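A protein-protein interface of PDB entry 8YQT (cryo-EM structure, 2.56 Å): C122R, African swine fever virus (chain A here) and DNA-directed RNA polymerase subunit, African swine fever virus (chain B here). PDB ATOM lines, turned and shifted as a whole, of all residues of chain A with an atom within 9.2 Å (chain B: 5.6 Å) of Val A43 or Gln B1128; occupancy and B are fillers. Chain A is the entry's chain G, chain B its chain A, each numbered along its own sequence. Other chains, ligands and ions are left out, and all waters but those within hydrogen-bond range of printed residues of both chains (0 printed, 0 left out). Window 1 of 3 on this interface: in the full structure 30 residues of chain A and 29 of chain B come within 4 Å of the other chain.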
ATOM      1  N   SER A  40      14.246  -3.973   7.921  1.00  0.00           N
ATOM      2  CA  SER A  40      13.231  -3.199   8.615  1.00  0.00           C
ATOM      3  C   SER A  40      13.821  -1.857   9.015  1.00  0.00           C
ATOM      4  O   SER A  40      15.035  -1.651   8.961  1.00  0.00           O
ATOM      5  CB  SER A  40      12.693  -3.947   9.842  1.00  0.00           C
ATOM      6  OG  SER A  40      11.722  -3.177  10.527  1.00  0.00           O
ATOM      7  N   SER A  41      12.945  -0.941   9.417  1.00  0.00           N
ATOM      8  CA  SER A  41      13.373   0.410   9.741  1.00  0.00           C
ATOM      9  C   SER A  41      12.375   1.047  10.694  1.00  0.00           C
ATOM     10  O   SER A  41      11.238   0.591  10.834  1.00  0.00           O
ATOM     11  CB  SER A  41      13.519   1.265   8.481  1.00  0.00           C
ATOM     12  OG  SER A  41      14.525   2.242   8.652  1.00  0.00           O
ATOM     13  N   LYS A  42      12.828   2.111  11.354  1.00  0.00           N
ATOM     14  CA  LYS A  42      11.961   2.942  12.175  1.00  0.00           C
ATOM     15  C   LYS A  42      12.632   4.289  12.379  1.00  0.00           C
ATOM     16  O   LYS A  42      13.832   4.353  12.651  1.00  0.00           O
ATOM     17  CB  LYS A  42      11.662   2.288  13.528  1.00  0.00           C
ATOM     18  CG  LYS A  42      10.916   3.180  14.503  1.00  0.00           C
ATOM     19  CD  LYS A  42       9.604   2.546  14.932  1.00  0.00           C
ATOM     20  CE  LYS A  42       9.051   3.215  16.177  1.00  0.00           C
ATOM     21  NZ  LYS A  42       7.606   2.923  16.372  1.00  0.00           N
ATOM     22  N   VAL A  43      11.853   5.357  12.238  1.00  0.00           N
ATOM     23  CA  VAL A  43      12.307   6.715  12.501  1.00  0.00           C
ATOM     24  C   VAL A  43      11.490   7.267  13.660  1.00  0.00           C
ATOM     25  O   VAL A  43      10.316   6.919  13.829  1.00  0.00           O
ATOM     26  CB  VAL A  43      12.204   7.611  11.245  1.00  0.00           C
ATOM     27  CG1 VAL A  43      10.824   8.218  11.109  1.00  0.00           C
ATOM     28  CG2 VAL A  43      13.253   8.710  11.286  1.00  0.00           C
ATOM     29  N   TYR A  44      12.125   8.096  14.480  1.00  0.00           N
ATOM     30  CA  TYR A  44      11.522   8.600  15.704  1.00  0.00           C
ATOM     31  C   TYR A  44      11.238  10.090  15.588  1.00  0.00           C
ATOM     32  O   TYR A  44      11.800  10.790  14.741  1.00  0.00           O
ATOM     33  CB  TYR A  44      12.428   8.327  16.907  1.00  0.00           C
ATOM     34  CG  TYR A  44      12.587   6.859  17.209  1.00  0.00           C
ATOM     35  CD1 TYR A  44      11.652   6.185  17.978  1.00  0.00           C
ATOM     36  CD2 TYR A  44      13.663   6.143  16.711  1.00  0.00           C
ATOM     37  CE1 TYR A  44      11.789   4.845  18.251  1.00  0.00           C
ATOM     38  CE2 TYR A  44      13.808   4.800  16.979  1.00  0.00           C
ATOM     39  CZ  TYR A  44      12.868   4.156  17.749  1.00  0.00           C
ATOM     40  OH  TYR A  44      13.005   2.816  18.021  1.00  0.00           O
ATOM     41  N   HIS A  45      10.353  10.565  16.465  1.00  0.00           N
ATOM     42  CA  HIS A  45       9.929  11.964  16.493  1.00  0.00           C
ATOM     43  C   HIS A  45       9.359  12.382  15.139  1.00  0.00           C
ATOM     44  O   HIS A  45       9.731  13.408  14.567  1.00  0.00           O
ATOM     45  CB  HIS A  45      11.079  12.882  16.915  1.00  0.00           C
ATOM     46  CG  HIS A  45      11.684  12.523  18.237  1.00  0.00           C
ATOM     47  ND1 HIS A  45      12.809  11.736  18.350  1.00  0.00           N
ATOM     48  CD2 HIS A  45      11.319  12.840  19.501  1.00  0.00           C
ATOM     49  CE1 HIS A  45      13.113  11.586  19.626  1.00  0.00           C
ATOM     50  NE2 HIS A  45      12.223  12.245  20.346  1.00  0.00           N
ATOM     51  N   THR A  46       8.448  11.556  14.621  1.00  0.00           N
ATOM     52  CA  THR A  46       7.879  11.792  13.300  1.00  0.00           C
ATOM     53  C   THR A  46       7.007  13.037  13.262  1.00  0.00           C
ATOM     54  O   THR A  46       6.909  13.688  12.215  1.00  0.00           O
ATOM     55  CB  THR A  46       7.065  10.578  12.855  1.00  0.00           C
ATOM     56  OG1 THR A  46       6.006  10.345  13.791  1.00  0.00           O
ATOM     57  CG2 THR A  46       7.940   9.350  12.799  1.00  0.00           C
ATOM     58  N   GLY A  47       6.377  13.389  14.379  1.00  0.00           N
ATOM     59  CA  GLY A  47       5.527  14.555  14.440  1.00  0.00           C
ATOM     60  C   GLY A  47       6.252  15.866  14.610  1.00  0.00           C
ATOM     61  O   GLY A  47       5.607  16.893  14.834  1.00  0.00           O
ATOM     62  N   GLU A  48       7.585  15.866  14.517  1.00  0.00           N
ATOM     63  CA  GLU A  48       8.357  17.090  14.686  1.00  0.00           C
ATOM     64  C   GLU A  48       9.490  17.230  13.675  1.00  0.00           C
ATOM     65  O   GLU A  48      10.303  18.153  13.810  1.00  0.00           O
ATOM     66  CB  GLU A  48       8.936  17.167  16.106  1.00  0.00           C
ATOM     67  CG  GLU A  48       7.894  17.236  17.206  1.00  0.00           C
ATOM     68  CD  GLU A  48       8.504  17.183  18.592  1.00  0.00           C
ATOM     69  OE1 GLU A  48       9.748  17.174  18.694  1.00  0.00           O
ATOM     70  OE2 GLU A  48       7.737  17.143  19.575  1.00  0.00           O
ATOM     71  N   MET A  49       9.577  16.358  12.673  1.00  0.00           N
ATOM     72  CA  MET A  49      10.703  16.392  11.753  1.00  0.00           C
ATOM     73  C   MET A  49      10.543  17.531  10.747  1.00  0.00           C
ATOM     74  O   MET A  49       9.523  18.224  10.701  1.00  0.00           O
ATOM     75  CB  MET A  49      10.855  15.055  11.032  1.00  0.00           C
ATOM     76  CG  MET A  49       9.579  14.514  10.419  1.00  0.00           C
ATOM     77  SD  MET A  49       9.595  12.716  10.300  1.00  0.00           S
ATOM     78  CE  MET A  49       8.142  12.428   9.299  1.00  0.00           C
ATOM     79  N   ASP A  51      10.568  17.194   7.364  1.00  0.00           N
ATOM     80  CA  ASP A  51       9.704  16.796   6.261  1.00  0.00           C
ATOM     81  C   ASP A  51       8.228  16.827   6.629  1.00  0.00           C
ATOM     82  O   ASP A  51       7.384  16.781   5.729  1.00  0.00           O
ATOM     83  CB  ASP A  51      10.086  15.397   5.774  1.00  0.00           C
ATOM     84  CG  ASP A  51      11.377  15.389   4.977  1.00  0.00           C
ATOM     85  OD1 ASP A  51      11.621  16.358   4.228  1.00  0.00           O
ATOM     86  OD2 ASP A  51      12.153  14.418   5.106  1.00  0.00           O
ATOM     87  N   ILE B1126      17.754   7.744  20.104  1.00  0.00           N
ATOM     88  CA  ILE B1126      17.823   7.321  18.710  1.00  0.00           C
ATOM     89  C   ILE B1126      16.878   8.181  17.885  1.00  0.00           C
ATOM     90  O   ILE B1126      15.728   8.404  18.278  1.00  0.00           O
ATOM     91  CB  ILE B1126      17.468   5.830  18.567  1.00  0.00           C
ATOM     92  CG1 ILE B1126      18.456   4.969  19.347  1.00  0.00           C
ATOM     93  CG2 ILE B1126      17.455   5.415  17.118  1.00  0.00           C
ATOM     94  CD1 ILE B1126      19.890   5.269  19.025  1.00  0.00           C
ATOM     95  N   LEU B1127      17.369   8.674  16.745  1.00  0.00           N
ATOM     96  CA  LEU B1127      16.486   9.293  15.763  1.00  0.00           C
ATOM     97  C   LEU B1127      15.881   8.244  14.838  1.00  0.00           C
ATOM     98  O   LEU B1127      14.681   8.280  14.544  1.00  0.00           O
ATOM     99  CB  LEU B1127      17.242  10.346  14.953  1.00  0.00           C
ATOM    100  CG  LEU B1127      17.178  11.789  15.453  1.00  0.00           C
ATOM    101  CD1 LEU B1127      18.059  12.686  14.607  1.00  0.00           C
ATOM    102  CD2 LEU B1127      15.747  12.292  15.459  1.00  0.00           C
ATOM    103  N   GLN B1128      16.695   7.299  14.374  1.00  0.00           N
ATOM    104  CA  GLN B1128      16.215   6.249  13.490  1.00  0.00           C
ATOM    105  C   GLN B1128      17.150   5.054  13.571  1.00  0.00           C
ATOM    106  O   GLN B1128      18.338   5.191  13.878  1.00  0.00           O
ATOM    107  CB  GLN B1128      16.106   6.744  12.045  1.00  0.00           C
ATOM    108  CG  GLN B1128      17.428   7.112  11.410  1.00  0.00           C
ATOM    109  CD  GLN B1128      17.256   7.848  10.101  1.00  0.00           C
ATOM    110  OE1 GLN B1128      16.136   8.068   9.642  1.00  0.00           O
ATOM    111  NE2 GLN B1128      18.368   8.235   9.489  1.00  0.00           N
ATOM    112  N   TRP B1129      16.601   3.872  13.294  1.00  0.00           N
ATOM    113  CA  TRP B1129      17.408   2.664  13.211  1.00  0.00           C
ATOM    114  C   TRP B1129      17.048   1.883  11.956  1.00  0.00           C
ATOM    115  O   TRP B1129      15.891   1.844  11.532  1.00  0.00           O
ATOM    116  CB  TRP B1129      17.265   1.769  14.455  1.00  0.00           C
ATOM    117  CG  TRP B1129      15.872   1.343  14.812  1.00  0.00           C
ATOM    118  CD1 TRP B1129      15.055   1.922  15.732  1.00  0.00           C
ATOM    119  CD2 TRP B1129      15.152   0.222  14.284  1.00  0.00           C
ATOM    120  NE1 TRP B1129      13.864   1.245  15.800  1.00  0.00           N
ATOM    121  CE2 TRP B1129      13.899   0.195  14.921  1.00  0.00           C
ATOM    122  CE3 TRP B1129      15.442  -0.755  13.328  1.00  0.00           C
ATOM    123  CZ2 TRP B1129      12.937  -0.766  14.633  1.00  0.00           C
ATOM    124  CZ3 TRP B1129      14.489  -1.707  13.045  1.00  0.00           C
ATOM    125  CH2 TRP B1129      13.251  -1.707  13.693  1.00  0.00           C
ATOM    126  N   HIS B1130      18.068   1.262  11.367  1.00  0.00           N
ATOM    127  CA  HIS B1130      17.946   0.489  10.140  1.00  0.00           C
ATOM    128  C   HIS B1130      18.490  -0.907  10.394  1.00  0.00           C
ATOM    129  O   HIS B1130      19.616  -1.054  10.879  1.00  0.00           O
ATOM    130  CB  HIS B1130      18.729   1.147   9.000  1.00  0.00           C
ATOM    131  CG  HIS B1130      18.092   2.387   8.454  1.00  0.00           C
ATOM    132  ND1 HIS B1130      16.992   2.360   7.624  1.00  0.00           N
ATOM    133  CD2 HIS B1130      18.393   3.694   8.637  1.00  0.00           C
ATOM    134  CE1 HIS B1130      16.656   3.597   7.303  1.00  0.00           C
ATOM    135  NE2 HIS B1130      17.486   4.425   7.909  1.00  0.00           N
ATOM    136  N   ARG B1177      21.838  -0.405  12.127  1.00  0.00           N
ATOM    137  CA  ARG B1177      22.423   0.923  12.023  1.00  0.00           C
ATOM    138  C   ARG B1177      21.571   1.908  12.810  1.00  0.00           C
ATOM    139  O   ARG B1177      20.343   1.911  12.693  1.00  0.00           O
ATOM    140  CB  ARG B1177      22.524   1.356  10.561  1.00  0.00           C
ATOM    141  CG  ARG B1177      23.295   2.637  10.335  1.00  0.00           C
ATOM    142  CD  ARG B1177      23.314   2.989   8.865  1.00  0.00           C
ATOM    143  NE  ARG B1177      24.103   4.181   8.588  1.00  0.00           N
ATOM    144  CZ  ARG B1177      23.625   5.417   8.604  1.00  0.00           C
ATOM    145  NH1 ARG B1177      22.361   5.664   8.903  1.00  0.00           N
ATOM    146  NH2 ARG B1177      24.433   6.429   8.309  1.00  0.00           N
ATOM    147  N   LEU B1178      22.227   2.738  13.617  1.00  0.00           N
ATOM    148  CA  LEU B1178      21.535   3.614  14.555  1.00  0.00           C
ATOM    149  C   LEU B1178      21.969   5.050  14.325  1.00  0.00           C
ATOM    150  O   LEU B1178      23.155   5.319  14.114  1.00  0.00           O
ATOM    151  CB  LEU B1178      21.816   3.193  15.994  1.00  0.00           C
ATOM    152  CG  LEU B1178      21.376   1.769  16.306  1.00  0.00           C
ATOM    153  CD1 LEU B1178      22.275   1.198  17.358  1.00  0.00           C
ATOM    154  CD2 LEU B1178      19.943   1.762  16.784  1.00  0.00           C
ATOM    155  N   GLU B1179      21.005   5.962  14.372  1.00  0.00           N
ATOM    156  CA  GLU B1179      21.240   7.386  14.185  1.00  0.00           C
ATOM    157  C   GLU B1179      20.882   8.114  15.476  1.00  0.00           C
ATOM    158  O   GLU B1179      19.711   8.148  15.868  1.00  0.00           O
ATOM    159  CB  GLU B1179      20.412   7.899  13.009  1.00  0.00           C
ATOM    160  CG  GLU B1179      21.124   8.837  12.062  1.00  0.00           C
ATOM    161  CD  GLU B1179      20.842  10.287  12.377  1.00  0.00           C
ATOM    162  OE1 GLU B1179      19.793  10.566  12.992  1.00  0.00           O
ATOM    163  OE2 GLU B1179      21.648  11.152  11.992  1.00  0.00           O
ATOM    164  N   LEU B1180      21.886   8.693  16.128  1.00  0.00           N
ATOM    165  CA  LEU B1180      21.693   9.299  17.437  1.00  0.00           C
ATOM    166  C   LEU B1180      21.087  10.690  17.321  1.00  0.00           C
ATOM    167  O   LEU B1180      21.445  11.472  16.437  1.00  0.00           O
ATOM    168  CB  LEU B1180      23.020   9.381  18.190  1.00  0.00           C
ATOM    169  CG  LEU B1180      23.629   8.063  18.659  1.00  0.00           C
ATOM    170  CD1 LEU B1180      25.003   8.308  19.233  1.00  0.00           C
ATOM    171  CD2 LEU B1180      22.737   7.399  19.686  1.00  0.00           C
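A ring nitrogen (ND1) of His B1130 is in hydrogen-bond range of the side-chain hydroxyl of Ser A41 (2.7 Å).
NE1 of Trp B1129 sits at hydrogen-bond distance from OH of Tyr A44 (2.9 Å).
O of Trp B1129 sits at hydrogen-bond distance from OG of Ser A41 (3.2 Å).
The backbone NH (N) of Trp B1129 sits at hydrogen-bond distance from the backbone carbonyl oxygen (O) of Lys A42, 2.9 Å away.
The backbone NH of Tyr A44 is in hydrogen-bond range of the backbone carbonyl oxygen of Leu B1127, 2.6 Å away.
N of Arg B1177 lies within hydrogen-bond range of O of His B1130, 2.6 Å away.
The backbone NH (N) of Leu B1127 sits at hydrogen-bond distance from the backbone carbonyl oxygen (O) of Glu B1179.
N of Glu B1179 lies within hydrogen-bond range of O of Gln B1128, at 2.8 Å.
Among the printed residues, pairs that only touch across the chains: Ser A40 with Trp B1129, Ser A40 with His B1130, Lys A42 with Gln B1128, Val A43 with Leu B1127, Val A43 with Gln B1128, Tyr A44 with Ile B1126 and Tyr A44 with Gln B1128.
Of the printed residues of chain B, Ser A40 touches Trp B1129 and His B1130.
Printed residues of chain B within 4 Å of Lys A42: Gln B1128 and Trp B1129.
Of chain B, only Leu B1127 (3.5 Å) and Gln B1128 (3.4 Å) come within 4 Å of Val A43.
Printed residues of chain B within 4 Å of Tyr A44: Ile B1126 (3.4 Å), Leu B1127 (2.6 Å), Gln B1128 (3.999 Å) and Trp B1129 (2.9 Å).
Gly A47 touches none of the printed residues of chain B.
Glu A48 touches none of the printed residues of chain B.
Printed residues of chain A within 4 Å of Leu B1127: Val A43 (3.5 Å) and Tyr A44 (2.6 Å).
Printed residues of chain A within 4 Å of Gln B1128: Lys A42 (3.2 Å), Val A43 (3.4 Å) and Tyr A44 (3.999 Å).
Of the printed residues of chain A, Trp B1129 touches Ser A40, Ser A41, Lys A42 and Tyr A44.
The nearest residue of chain B that does not touch Val A43 is Trp B1129 (5.1 Å).
The nearest printed residue of chain A that does not touch Gln B1128 is Ser A41 (5.9 Å).
The nearest printed residue of chain A that does not touch His B1130 is Lys A42 (5.3 Å).
Of the 9 printed residues of chain B, 5 touch a printed residue of chain A.
Among the printed residues, no Asp or Glu carboxylate lies within 4 Å of a Lys or Arg side-chain nitrogen of the other chain.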
